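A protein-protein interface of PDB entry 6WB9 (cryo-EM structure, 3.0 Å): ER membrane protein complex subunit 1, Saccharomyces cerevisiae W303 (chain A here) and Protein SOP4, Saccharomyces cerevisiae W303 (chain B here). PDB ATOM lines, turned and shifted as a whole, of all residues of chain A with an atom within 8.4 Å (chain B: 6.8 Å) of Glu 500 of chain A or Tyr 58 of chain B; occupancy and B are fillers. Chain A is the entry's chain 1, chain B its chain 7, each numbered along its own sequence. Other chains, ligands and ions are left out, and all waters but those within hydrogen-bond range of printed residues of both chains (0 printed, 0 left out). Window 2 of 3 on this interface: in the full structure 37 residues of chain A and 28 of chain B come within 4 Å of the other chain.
The side-chain hydroxyl (OH) of Tyr 58 of chain B is in hydrogen-bond range of the side-chain carboxylate (OE2) of Glu 500 of chain A (2.8 Å).
OH of Tyr 49 of chain B is in hydrogen-bond range of OD2 of Asp 528 of chain A.
O of Pro 59 of chain B is in hydrogen-bond range of NH1 of Arg 530 of chain A (2.5 Å).
NH1 of Arg 530 of chain A sits at hydrogen-bond distance from OG1 of Thr 61 of chain B, 2.8 Å away.
O of Lys 457 of chain A is in hydrogen-bond range of N of Glu 500 of chain A, 3.1 Å away.
O of Glu 500 of chain A sits at hydrogen-bond distance from NE2 of His 503 of chain A, 3.2 Å away.
The guanidinium group (NH1) of Arg 530 of chain A is in salt-bridge range of the side-chain carboxylate (OD2) of Asp 528 of chain A, at 2.6 Å.
The side-chain hydroxyl (OG1) of Thr 56 of chain B is in hydrogen-bond range of the backbone carbonyl oxygen (O) of Tyr 58 of chain B (2.7 Å).
Among the printed residues, merely in contact across the chains: Asp 528 of chain A with Tyr 58 of chain B, Asp 528 of chain A with Pro 59 of chain B, Arg 530 of chain A with Tyr 58 of chain B, Phe 531 of chain A with Tyr 49 of chain B and Phe 531 of chain A with Thr 61 of chain B.
Of chain B, only Tyr 58 comes within 4 Å of Glu 500 of chain A.
Printed residues of chain A within 4 Å of Tyr 58 of chain B: Glu 500 (2.8 Å), Asp 528 (3.5 Å) and Arg 530 (3.6 Å).
Pro 59 of chain B touches just these residues of chain A: Asp 528 (3.9 Å) and Arg 530 (2.5 Å).
Of the printed residues of chain B, Phe 531 of chain A touches Tyr 49 (3.9 Å) and Thr 61 (3.6 Å).
Of the printed residues of chain A, Tyr 49 of chain B touches Asp 528 (3.1 Å) and Phe 531 (3.9 Å).
The nearest printed residue of chain A that does not touch Tyr 58 of chain B is Phe 529 of chain A (4.001 Å).
The nearest printed residue of chain B that does not touch Asp 528 of chain A is Thr 61 of chain B (4.1 Å).
Printed residues of chain A that touch a printed residue of chain B: Glu 500, Asp 528, Arg 530 and Phe 531.
Hydrophobic or aromatic side chains of chain B within 4 Å of the printed part of chain A: Tyr 49, Tyr 58 and Pro 59.
Along chain B the printed residues that touch a printed residue of chain A span positions 49 to 61.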
ATOM      1  N   ASN A 455     -39.389  -7.736  24.400  1.00  0.00           N
ATOM      2  CA  ASN A 455     -39.220  -9.115  23.969  1.00  0.00           C
ATOM      3  C   ASN A 455     -38.205  -9.814  24.871  1.00  0.00           C
ATOM      4  O   ASN A 455     -37.819  -9.302  25.924  1.00  0.00           O
ATOM      5  CB  ASN A 455     -38.829  -9.172  22.494  1.00  0.00           C
ATOM      6  CG  ASN A 455     -37.710  -8.220  22.147  1.00  0.00           C
ATOM      7  OD1 ASN A 455     -37.944  -7.041  21.895  1.00  0.00           O
ATOM      8  ND2 ASN A 455     -36.488  -8.731  22.110  1.00  0.00           N
ATOM      9  N   SER A 456     -37.770 -11.007  24.467  1.00  0.00           N
ATOM     10  CA  SER A 456     -36.931 -11.836  25.324  1.00  0.00           C
ATOM     11  C   SER A 456     -35.494 -11.347  25.406  1.00  0.00           C
ATOM     12  O   SER A 456     -34.812 -11.637  26.394  1.00  0.00           O
ATOM     13  CB  SER A 456     -36.951 -13.283  24.829  1.00  0.00           C
ATOM     14  OG  SER A 456     -38.271 -13.800  24.819  1.00  0.00           O
ATOM     15  N   LYS A 457     -35.021 -10.611  24.405  1.00  0.00           N
ATOM     16  CA  LYS A 457     -33.652 -10.119  24.387  1.00  0.00           C
ATOM     17  C   LYS A 457     -33.528  -8.694  24.903  1.00  0.00           C
ATOM     18  O   LYS A 457     -32.412  -8.175  24.983  1.00  0.00           O
ATOM     19  CB  LYS A 457     -33.084 -10.202  22.969  1.00  0.00           C
ATOM     20  CG  LYS A 457     -33.029 -11.606  22.398  1.00  0.00           C
ATOM     21  CD  LYS A 457     -32.111 -12.501  23.213  1.00  0.00           C
ATOM     22  CE  LYS A 457     -32.100 -13.917  22.667  1.00  0.00           C
ATOM     23  NZ  LYS A 457     -33.465 -14.513  22.653  1.00  0.00           N
ATOM     24  N   GLU A 458     -34.635  -8.054  25.257  1.00  0.00           N
ATOM     25  CA  GLU A 458     -34.633  -6.672  25.703  1.00  0.00           C
ATOM     26  C   GLU A 458     -34.961  -6.589  27.185  1.00  0.00           C
ATOM     27  O   GLU A 458     -35.503  -7.519  27.788  1.00  0.00           O
ATOM     28  CB  GLU A 458     -35.627  -5.840  24.889  1.00  0.00           C
ATOM     29  CG  GLU A 458     -35.272  -5.742  23.425  1.00  0.00           C
ATOM     30  CD  GLU A 458     -35.996  -4.618  22.721  1.00  0.00           C
ATOM     31  OE1 GLU A 458     -37.198  -4.420  22.993  1.00  0.00           O
ATOM     32  OE2 GLU A 458     -35.357  -3.917  21.908  1.00  0.00           O
ATOM     33  N   LYS A 459     -34.623  -5.444  27.771  1.00  0.00           N
ATOM     34  CA  LYS A 459     -34.840  -5.223  29.193  1.00  0.00           C
ATOM     35  C   LYS A 459     -34.971  -3.730  29.440  1.00  0.00           C
ATOM     36  O   LYS A 459     -34.124  -2.960  28.993  1.00  0.00           O
ATOM     37  CB  LYS A 459     -33.681  -5.800  30.011  1.00  0.00           C
ATOM     38  CG  LYS A 459     -33.760  -5.542  31.502  1.00  0.00           C
ATOM     39  CD  LYS A 459     -32.538  -6.098  32.211  1.00  0.00           C
ATOM     40  CE  LYS A 459     -32.626  -5.907  33.717  1.00  0.00           C
ATOM     41  NZ  LYS A 459     -32.674  -4.472  34.103  1.00  0.00           N
ATOM     42  N   VAL A 461     -34.214  -0.747  31.392  1.00  0.00           N
ATOM     43  CA  VAL A 461     -33.100  -0.532  32.308  1.00  0.00           C
ATOM     44  C   VAL A 461     -33.174   0.796  33.038  1.00  0.00           C
ATOM     45  O   VAL A 461     -32.484   0.961  34.057  1.00  0.00           O
ATOM     46  CB  VAL A 461     -31.749  -0.655  31.578  1.00  0.00           C
ATOM     47  CG1 VAL A 461     -31.372  -2.111  31.423  1.00  0.00           C
ATOM     48  CG2 VAL A 461     -31.849  -0.005  30.232  1.00  0.00           C
ATOM     49  N   ILE A 497     -34.520   1.050  26.823  1.00  0.00           N
ATOM     50  CA  ILE A 497     -34.616  -0.372  26.533  1.00  0.00           C
ATOM     51  C   ILE A 497     -33.239  -0.842  26.099  1.00  0.00           C
ATOM     52  O   ILE A 497     -32.711  -0.379  25.083  1.00  0.00           O
ATOM     53  CB  ILE A 497     -35.662  -0.661  25.449  1.00  0.00           C
ATOM     54  CG1 ILE A 497     -37.032  -0.160  25.884  1.00  0.00           C
ATOM     55  CG2 ILE A 497     -35.725  -2.131  25.171  1.00  0.00           C
ATOM     56  CD1 ILE A 497     -37.545  -0.836  27.119  1.00  0.00           C
ATOM     57  N   ALA A 498     -32.654  -1.750  26.863  1.00  0.00           N
ATOM     58  CA  ALA A 498     -31.374  -2.346  26.527  1.00  0.00           C
ATOM     59  C   ALA A 498     -31.633  -3.604  25.715  1.00  0.00           C
ATOM     60  O   ALA A 498     -32.351  -4.501  26.170  1.00  0.00           O
ATOM     61  CB  ALA A 498     -30.583  -2.670  27.792  1.00  0.00           C
ATOM     62  N   ASN A 499     -31.067  -3.662  24.512  1.00  0.00           N
ATOM     63  CA  ASN A 499     -31.209  -4.811  23.627  1.00  0.00           C
ATOM     64  C   ASN A 499     -29.863  -5.517  23.562  1.00  0.00           C
ATOM     65  O   ASN A 499     -28.900  -4.977  23.005  1.00  0.00           O
ATOM     66  CB  ASN A 499     -31.677  -4.376  22.242  1.00  0.00           C
ATOM     67  CG  ASN A 499     -32.353  -5.491  21.473  1.00  0.00           C
ATOM     68  OD1 ASN A 499     -32.027  -6.664  21.632  1.00  0.00           O
ATOM     69  ND2 ASN A 499     -33.311  -5.125  20.635  1.00  0.00           N
ATOM     70  N   GLU A 500     -29.800  -6.719  24.139  1.00  0.00           N
ATOM     71  CA  GLU A 500     -28.588  -7.524  24.136  1.00  0.00           C
ATOM     72  C   GLU A 500     -28.389  -8.293  22.840  1.00  0.00           C
ATOM     73  O   GLU A 500     -27.269  -8.741  22.573  1.00  0.00           O
ATOM     74  CB  GLU A 500     -28.600  -8.507  25.309  1.00  0.00           C
ATOM     75  CG  GLU A 500     -28.551  -7.847  26.677  1.00  0.00           C
ATOM     76  CD  GLU A 500     -28.164  -8.814  27.783  1.00  0.00           C
ATOM     77  OE1 GLU A 500     -28.278 -10.041  27.574  1.00  0.00           O
ATOM     78  OE2 GLU A 500     -27.740  -8.347  28.862  1.00  0.00           O
ATOM     79  N   GLU A 501     -29.439  -8.465  22.037  1.00  0.00           N
ATOM     80  CA  GLU A 501     -29.296  -9.146  20.757  1.00  0.00           C
ATOM     81  C   GLU A 501     -28.594  -8.256  19.742  1.00  0.00           C
ATOM     82  O   GLU A 501     -27.645  -8.685  19.077  1.00  0.00           O
ATOM     83  CB  GLU A 501     -30.667  -9.574  20.238  1.00  0.00           C
ATOM     84  CG  GLU A 501     -30.649 -10.241  18.874  1.00  0.00           C
ATOM     85  CD  GLU A 501     -32.044 -10.533  18.356  1.00  0.00           C
ATOM     86  OE1 GLU A 501     -33.021 -10.242  19.079  1.00  0.00           O
ATOM     87  OE2 GLU A 501     -32.167 -11.051  17.227  1.00  0.00           O
ATOM     88  N   HIS A 502     -29.049  -7.013  19.611  1.00  0.00           N
ATOM     89  CA  HIS A 502     -28.424  -6.055  18.713  1.00  0.00           C
ATOM     90  C   HIS A 502     -27.423  -5.151  19.412  1.00  0.00           C
ATOM     91  O   HIS A 502     -26.711  -4.412  18.722  1.00  0.00           O
ATOM     92  CB  HIS A 502     -29.492  -5.193  18.039  1.00  0.00           C
ATOM     93  CG  HIS A 502     -30.531  -5.984  17.312  1.00  0.00           C
ATOM     94  ND1 HIS A 502     -30.403  -6.338  15.988  1.00  0.00           N
ATOM     95  CD2 HIS A 502     -31.711  -6.497  17.728  1.00  0.00           C
ATOM     96  CE1 HIS A 502     -31.462  -7.033  15.617  1.00  0.00           C
ATOM     97  NE2 HIS A 502     -32.273  -7.142  16.653  1.00  0.00           N
ATOM     98  N   HIS A 503     -27.350  -5.221  20.744  1.00  0.00           N
ATOM     99  CA  HIS A 503     -26.543  -4.347  21.600  1.00  0.00           C
ATOM    100  C   HIS A 503     -26.850  -2.875  21.315  1.00  0.00           C
ATOM    101  O   HIS A 503     -26.034  -2.131  20.779  1.00  0.00           O
ATOM    102  CB  HIS A 503     -25.044  -4.632  21.452  1.00  0.00           C
ATOM    103  CG  HIS A 503     -24.658  -6.038  21.785  1.00  0.00           C
ATOM    104  ND1 HIS A 503     -24.262  -6.946  20.829  1.00  0.00           N
ATOM    105  CD2 HIS A 503     -24.608  -6.692  22.969  1.00  0.00           C
ATOM    106  CE1 HIS A 503     -23.984  -8.100  21.409  1.00  0.00           C
ATOM    107  NE2 HIS A 503     -24.186  -7.972  22.707  1.00  0.00           N
ATOM    108  N   THR A 504     -28.088  -2.491  21.623  1.00  0.00           N
ATOM    109  CA  THR A 504     -28.533  -1.124  21.397  1.00  0.00           C
ATOM    110  C   THR A 504     -29.164  -0.553  22.657  1.00  0.00           C
ATOM    111  O   THR A 504     -29.656  -1.284  23.523  1.00  0.00           O
ATOM    112  CB  THR A 504     -29.552  -1.010  20.246  1.00  0.00           C
ATOM    113  OG1 THR A 504     -30.762  -1.688  20.599  1.00  0.00           O
ATOM    114  CG2 THR A 504     -29.018  -1.585  18.949  1.00  0.00           C
ATOM    115  N   ILE A 505     -29.150   0.774  22.741  1.00  0.00           N
ATOM    116  CA  ILE A 505     -29.883   1.520  23.761  1.00  0.00           C
ATOM    117  C   ILE A 505     -31.028   2.228  23.059  1.00  0.00           C
ATOM    118  O   ILE A 505     -30.799   3.063  22.181  1.00  0.00           O
ATOM    119  CB  ILE A 505     -28.995   2.532  24.494  1.00  0.00           C
ATOM    120  CG1 ILE A 505     -27.719   1.874  24.978  1.00  0.00           C
ATOM    121  CG2 ILE A 505     -29.729   3.106  25.681  1.00  0.00           C
ATOM    122  CD1 ILE A 505     -27.968   0.749  25.915  1.00  0.00           C
ATOM    123  N   PRO A 527     -22.793  -0.496  23.549  1.00  0.00           N
ATOM    124  CA  PRO A 527     -22.907  -0.154  24.965  1.00  0.00           C
ATOM    125  C   PRO A 527     -22.686  -1.363  25.862  1.00  0.00           C
ATOM    126  O   PRO A 527     -22.692  -2.514  25.425  1.00  0.00           O
ATOM    127  CB  PRO A 527     -24.341   0.347  25.069  1.00  0.00           C
ATOM    128  CG  PRO A 527     -25.047  -0.504  24.108  1.00  0.00           C
ATOM    129  CD  PRO A 527     -24.120  -0.735  22.965  1.00  0.00           C
ATOM    130  N   ASP A 528     -22.491  -1.074  27.144  1.00  0.00           N
ATOM    131  CA  ASP A 528     -22.296  -2.096  28.161  1.00  0.00           C
ATOM    132  C   ASP A 528     -23.441  -2.005  29.155  1.00  0.00           C
ATOM    133  O   ASP A 528     -23.674  -0.944  29.742  1.00  0.00           O
ATOM    134  CB  ASP A 528     -20.947  -1.927  28.860  1.00  0.00           C
ATOM    135  CG  ASP A 528     -20.421  -3.228  29.431  1.00  0.00           C
ATOM    136  OD1 ASP A 528     -21.231  -4.137  29.700  1.00  0.00           O
ATOM    137  OD2 ASP A 528     -19.194  -3.348  29.610  1.00  0.00           O
ATOM    138  N   PHE A 529     -24.154  -3.110  29.334  1.00  0.00           N
ATOM    139  CA  PHE A 529     -25.291  -3.164  30.236  1.00  0.00           C
ATOM    140  C   PHE A 529     -24.907  -3.595  31.644  1.00  0.00           C
ATOM    141  O   PHE A 529     -25.788  -3.721  32.499  1.00  0.00           O
ATOM    142  CB  PHE A 529     -26.356  -4.108  29.680  1.00  0.00           C
ATOM    143  CG  PHE A 529     -26.555  -3.988  28.200  1.00  0.00           C
ATOM    144  CD1 PHE A 529     -27.010  -2.810  27.643  1.00  0.00           C
ATOM    145  CD2 PHE A 529     -26.291  -5.058  27.363  1.00  0.00           C
ATOM    146  CE1 PHE A 529     -27.198  -2.701  26.283  1.00  0.00           C
ATOM    147  CE2 PHE A 529     -26.476  -4.948  25.999  1.00  0.00           C
ATOM    148  CZ  PHE A 529     -26.931  -3.766  25.462  1.00  0.00           C
ATOM    149  N   ARG A 530     -23.624  -3.821  31.904  1.00  0.00           N
ATOM    150  CA  ARG A 530     -23.139  -4.107  33.246  1.00  0.00           C
ATOM    151  C   ARG A 530     -22.859  -2.845  34.044  1.00  0.00           C
ATOM    152  O   ARG A 530     -22.448  -2.937  35.204  1.00  0.00           O
ATOM    153  CB  ARG A 530     -21.870  -4.955  33.178  1.00  0.00           C
ATOM    154  CG  ARG A 530     -22.036  -6.260  32.444  1.00  0.00           C
ATOM    155  CD  ARG A 530     -20.690  -6.901  32.215  1.00  0.00           C
ATOM    156  NE  ARG A 530     -19.834  -6.052  31.396  1.00  0.00           N
ATOM    157  CZ  ARG A 530     -18.564  -6.319  31.124  1.00  0.00           C
ATOM    158  NH1 ARG A 530     -17.858  -5.493  30.369  1.00  0.00           N
ATOM    159  NH2 ARG A 530     -18.001  -7.414  31.610  1.00  0.00           N
ATOM    160  N   PHE A 531     -23.067  -1.685  33.447  1.00  0.00           N
ATOM    161  CA  PHE A 531     -22.822  -0.378  34.019  1.00  0.00           C
ATOM    162  C   PHE A 531     -24.147   0.342  34.237  1.00  0.00           C
ATOM    163  O   PHE A 531     -25.139   0.031  33.571  1.00  0.00           O
ATOM    164  CB  PHE A 531     -21.914   0.426  33.081  1.00  0.00           C
ATOM    165  CG  PHE A 531     -20.489  -0.039  33.074  1.00  0.00           C
ATOM    166  CD1 PHE A 531     -19.554   0.548  33.904  1.00  0.00           C
ATOM    167  CD2 PHE A 531     -20.084  -1.067  32.244  1.00  0.00           C
ATOM    168  CE1 PHE A 531     -18.244   0.118  33.900  1.00  0.00           C
ATOM    169  CE2 PHE A 531     -18.775  -1.498  32.240  1.00  0.00           C
ATOM    170  CZ  PHE A 531     -17.858  -0.902  33.066  1.00  0.00           C
ATOM    171  N   TYR B  49     -10.784  -1.585  30.847  1.00  0.00           N
ATOM    172  CA  TYR B  49     -11.924  -1.871  29.983  1.00  0.00           C
ATOM    173  C   TYR B  49     -11.420  -2.308  28.617  1.00  0.00           C
ATOM    174  O   TYR B  49     -10.677  -1.569  27.966  1.00  0.00           O
ATOM    175  CB  TYR B  49     -12.830  -0.645  29.857  1.00  0.00           C
ATOM    176  CG  TYR B  49     -14.149  -0.935  29.194  1.00  0.00           C
ATOM    177  CD1 TYR B  49     -15.139  -1.633  29.864  1.00  0.00           C
ATOM    178  CD2 TYR B  49     -14.408  -0.509  27.901  1.00  0.00           C
ATOM    179  CE1 TYR B  49     -16.343  -1.908  29.267  1.00  0.00           C
ATOM    180  CE2 TYR B  49     -15.613  -0.777  27.293  1.00  0.00           C
ATOM    181  CZ  TYR B  49     -16.577  -1.477  27.982  1.00  0.00           C
ATOM    182  OH  TYR B  49     -17.785  -1.746  27.385  1.00  0.00           O
ATOM    183  N   GLN B  50     -11.831  -3.494  28.173  1.00  0.00           N
ATOM    184  CA  GLN B  50     -11.320  -4.057  26.929  1.00  0.00           C
ATOM    185  C   GLN B  50     -12.004  -3.431  25.723  1.00  0.00           C
ATOM    186  O   GLN B  50     -13.228  -3.277  25.703  1.00  0.00           O
ATOM    187  CB  GLN B  50     -11.525  -5.570  26.903  1.00  0.00           C
ATOM    188  CG  GLN B  50     -10.904  -6.247  25.697  1.00  0.00           C
ATOM    189  CD  GLN B  50     -11.109  -7.736  25.690  1.00  0.00           C
ATOM    190  OE1 GLN B  50     -11.936  -8.263  26.429  1.00  0.00           O
ATOM    191  NE2 GLN B  50     -10.354  -8.429  24.852  1.00  0.00           N
ATOM    192  N   PHE B  54     -12.792  -7.795  20.588  1.00  0.00           N
ATOM    193  CA  PHE B  54     -12.711  -8.938  21.482  1.00  0.00           C
ATOM    194  C   PHE B  54     -13.544 -10.098  20.937  1.00  0.00           C
ATOM    195  O   PHE B  54     -14.282  -9.966  19.958  1.00  0.00           O
ATOM    196  CB  PHE B  54     -13.168  -8.557  22.895  1.00  0.00           C
ATOM    197  CG  PHE B  54     -14.451  -7.768  22.940  1.00  0.00           C
ATOM    198  CD1 PHE B  54     -14.431  -6.380  22.941  1.00  0.00           C
ATOM    199  CD2 PHE B  54     -15.674  -8.415  23.008  1.00  0.00           C
ATOM    200  CE1 PHE B  54     -15.603  -5.658  22.977  1.00  0.00           C
ATOM    201  CE2 PHE B  54     -16.850  -7.697  23.049  1.00  0.00           C
ATOM    202  CZ  PHE B  54     -16.815  -6.317  23.036  1.00  0.00           C
ATOM    203  N   SER B  55     -13.426 -11.254  21.594  1.00  0.00           N
ATOM    204  CA  SER B  55     -14.053 -12.477  21.107  1.00  0.00           C
ATOM    205  C   SER B  55     -14.968 -13.116  22.145  1.00  0.00           C
ATOM    206  O   SER B  55     -15.289 -14.302  22.031  1.00  0.00           O
ATOM    207  CB  SER B  55     -12.992 -13.485  20.658  1.00  0.00           C
ATOM    208  OG  SER B  55     -13.588 -14.707  20.262  1.00  0.00           O
ATOM    209  N   THR B  56     -15.393 -12.363  23.150  1.00  0.00           N
ATOM    210  CA  THR B  56     -16.312 -12.848  24.167  1.00  0.00           C
ATOM    211  C   THR B  56     -17.653 -12.137  24.027  1.00  0.00           C
ATOM    212  O   THR B  56     -17.875 -11.351  23.103  1.00  0.00           O
ATOM    213  CB  THR B  56     -15.724 -12.651  25.564  1.00  0.00           C
ATOM    214  OG1 THR B  56     -15.280 -11.298  25.713  1.00  0.00           O
ATOM    215  CG2 THR B  56     -14.551 -13.590  25.779  1.00  0.00           C
ATOM    216  N   GLU B  57     -18.561 -12.436  24.958  1.00  0.00           N
ATOM    217  CA  GLU B  57     -19.864 -11.779  24.965  1.00  0.00           C
ATOM    218  C   GLU B  57     -19.729 -10.320  25.380  1.00  0.00           C
ATOM    219  O   GLU B  57     -20.092  -9.408  24.628  1.00  0.00           O
ATOM    220  CB  GLU B  57     -20.817 -12.523  25.900  1.00  0.00           C
ATOM    221  CG  GLU B  57     -22.241 -11.994  25.886  1.00  0.00           C
ATOM    222  CD  GLU B  57     -23.123 -12.667  26.919  1.00  0.00           C
ATOM    223  OE1 GLU B  57     -22.642 -12.911  28.045  1.00  0.00           O
ATOM    224  OE2 GLU B  57     -24.297 -12.957  26.602  1.00  0.00           O
ATOM    225  N   TYR B  58     -19.211 -10.087  26.552  1.00  0.00           N
ATOM    226  CA  TYR B  58     -18.932  -8.785  27.125  1.00  0.00           C
ATOM    227  C   TYR B  58     -17.438  -8.493  27.074  1.00  0.00           C
ATOM    228  O   TYR B  58     -16.618  -9.410  27.170  1.00  0.00           O
ATOM    229  CB  TYR B  58     -19.402  -8.722  28.580  1.00  0.00           C
ATOM    230  CG  TYR B  58     -20.896  -8.618  28.764  1.00  0.00           C
ATOM    231  CD1 TYR B  58     -21.566  -7.437  28.477  1.00  0.00           C
ATOM    232  CD2 TYR B  58     -21.631  -9.691  29.251  1.00  0.00           C
ATOM    233  CE1 TYR B  58     -22.932  -7.329  28.655  1.00  0.00           C
ATOM    234  CE2 TYR B  58     -22.999  -9.594  29.433  1.00  0.00           C
ATOM    235  CZ  TYR B  58     -23.643  -8.411  29.133  1.00  0.00           C
ATOM    236  OH  TYR B  58     -25.003  -8.306  29.312  1.00  0.00           O
ATOM    237  N   PRO B  59     -17.048  -7.231  26.909  1.00  0.00           N
ATOM    238  CA  PRO B  59     -15.633  -6.882  27.051  1.00  0.00           C
ATOM    239  C   PRO B  59     -15.190  -7.013  28.495  1.00  0.00           C
ATOM    240  O   PRO B  59     -15.986  -6.883  29.426  1.00  0.00           O
ATOM    241  CB  PRO B  59     -15.576  -5.427  26.580  1.00  0.00           C
ATOM    242  CG  PRO B  59     -16.940  -4.918  26.785  1.00  0.00           C
ATOM    243  CD  PRO B  59     -17.862  -6.066  26.529  1.00  0.00           C
ATOM    244  N   TYR B  60     -13.903  -7.285  28.677  1.00  0.00           N
ATOM    245  CA  TYR B  60     -13.369  -7.538  30.006  1.00  0.00           C
ATOM    246  C   TYR B  60     -13.249  -6.230  30.774  1.00  0.00           C
ATOM    247  O   TYR B  60     -12.614  -5.282  30.301  1.00  0.00           O
ATOM    248  CB  TYR B  60     -12.017  -8.235  29.919  1.00  0.00           C
ATOM    249  CG  TYR B  60     -11.448  -8.597  31.268  1.00  0.00           C
ATOM    250  CD1 TYR B  60     -11.958  -9.669  31.989  1.00  0.00           C
ATOM    251  CD2 TYR B  60     -10.409  -7.866  31.822  1.00  0.00           C
ATOM    252  CE1 TYR B  60     -11.444 -10.003  33.223  1.00  0.00           C
ATOM    253  CE2 TYR B  60      -9.896  -8.189  33.054  1.00  0.00           C
ATOM    254  CZ  TYR B  60     -10.412  -9.259  33.749  1.00  0.00           C
ATOM    255  OH  TYR B  60      -9.892  -9.583  34.980  1.00  0.00           O
ATOM    256  N   THR B  61     -13.859  -6.179  31.953  1.00  0.00           N
ATOM    257  CA  THR B  61     -13.783  -5.026  32.836  1.00  0.00           C
ATOM    258  C   THR B  61     -13.243  -5.471  34.183  1.00  0.00           C
ATOM    259  O   THR B  61     -13.772  -6.407  34.790  1.00  0.00           O
ATOM    260  CB  THR B  61     -15.148  -4.369  33.020  1.00  0.00           C
ATOM    261  OG1 THR B  61     -15.759  -4.168  31.743  1.00  0.00           O
ATOM    262  CG2 THR B  61     -14.990  -3.031  33.708  1.00  0.00           C
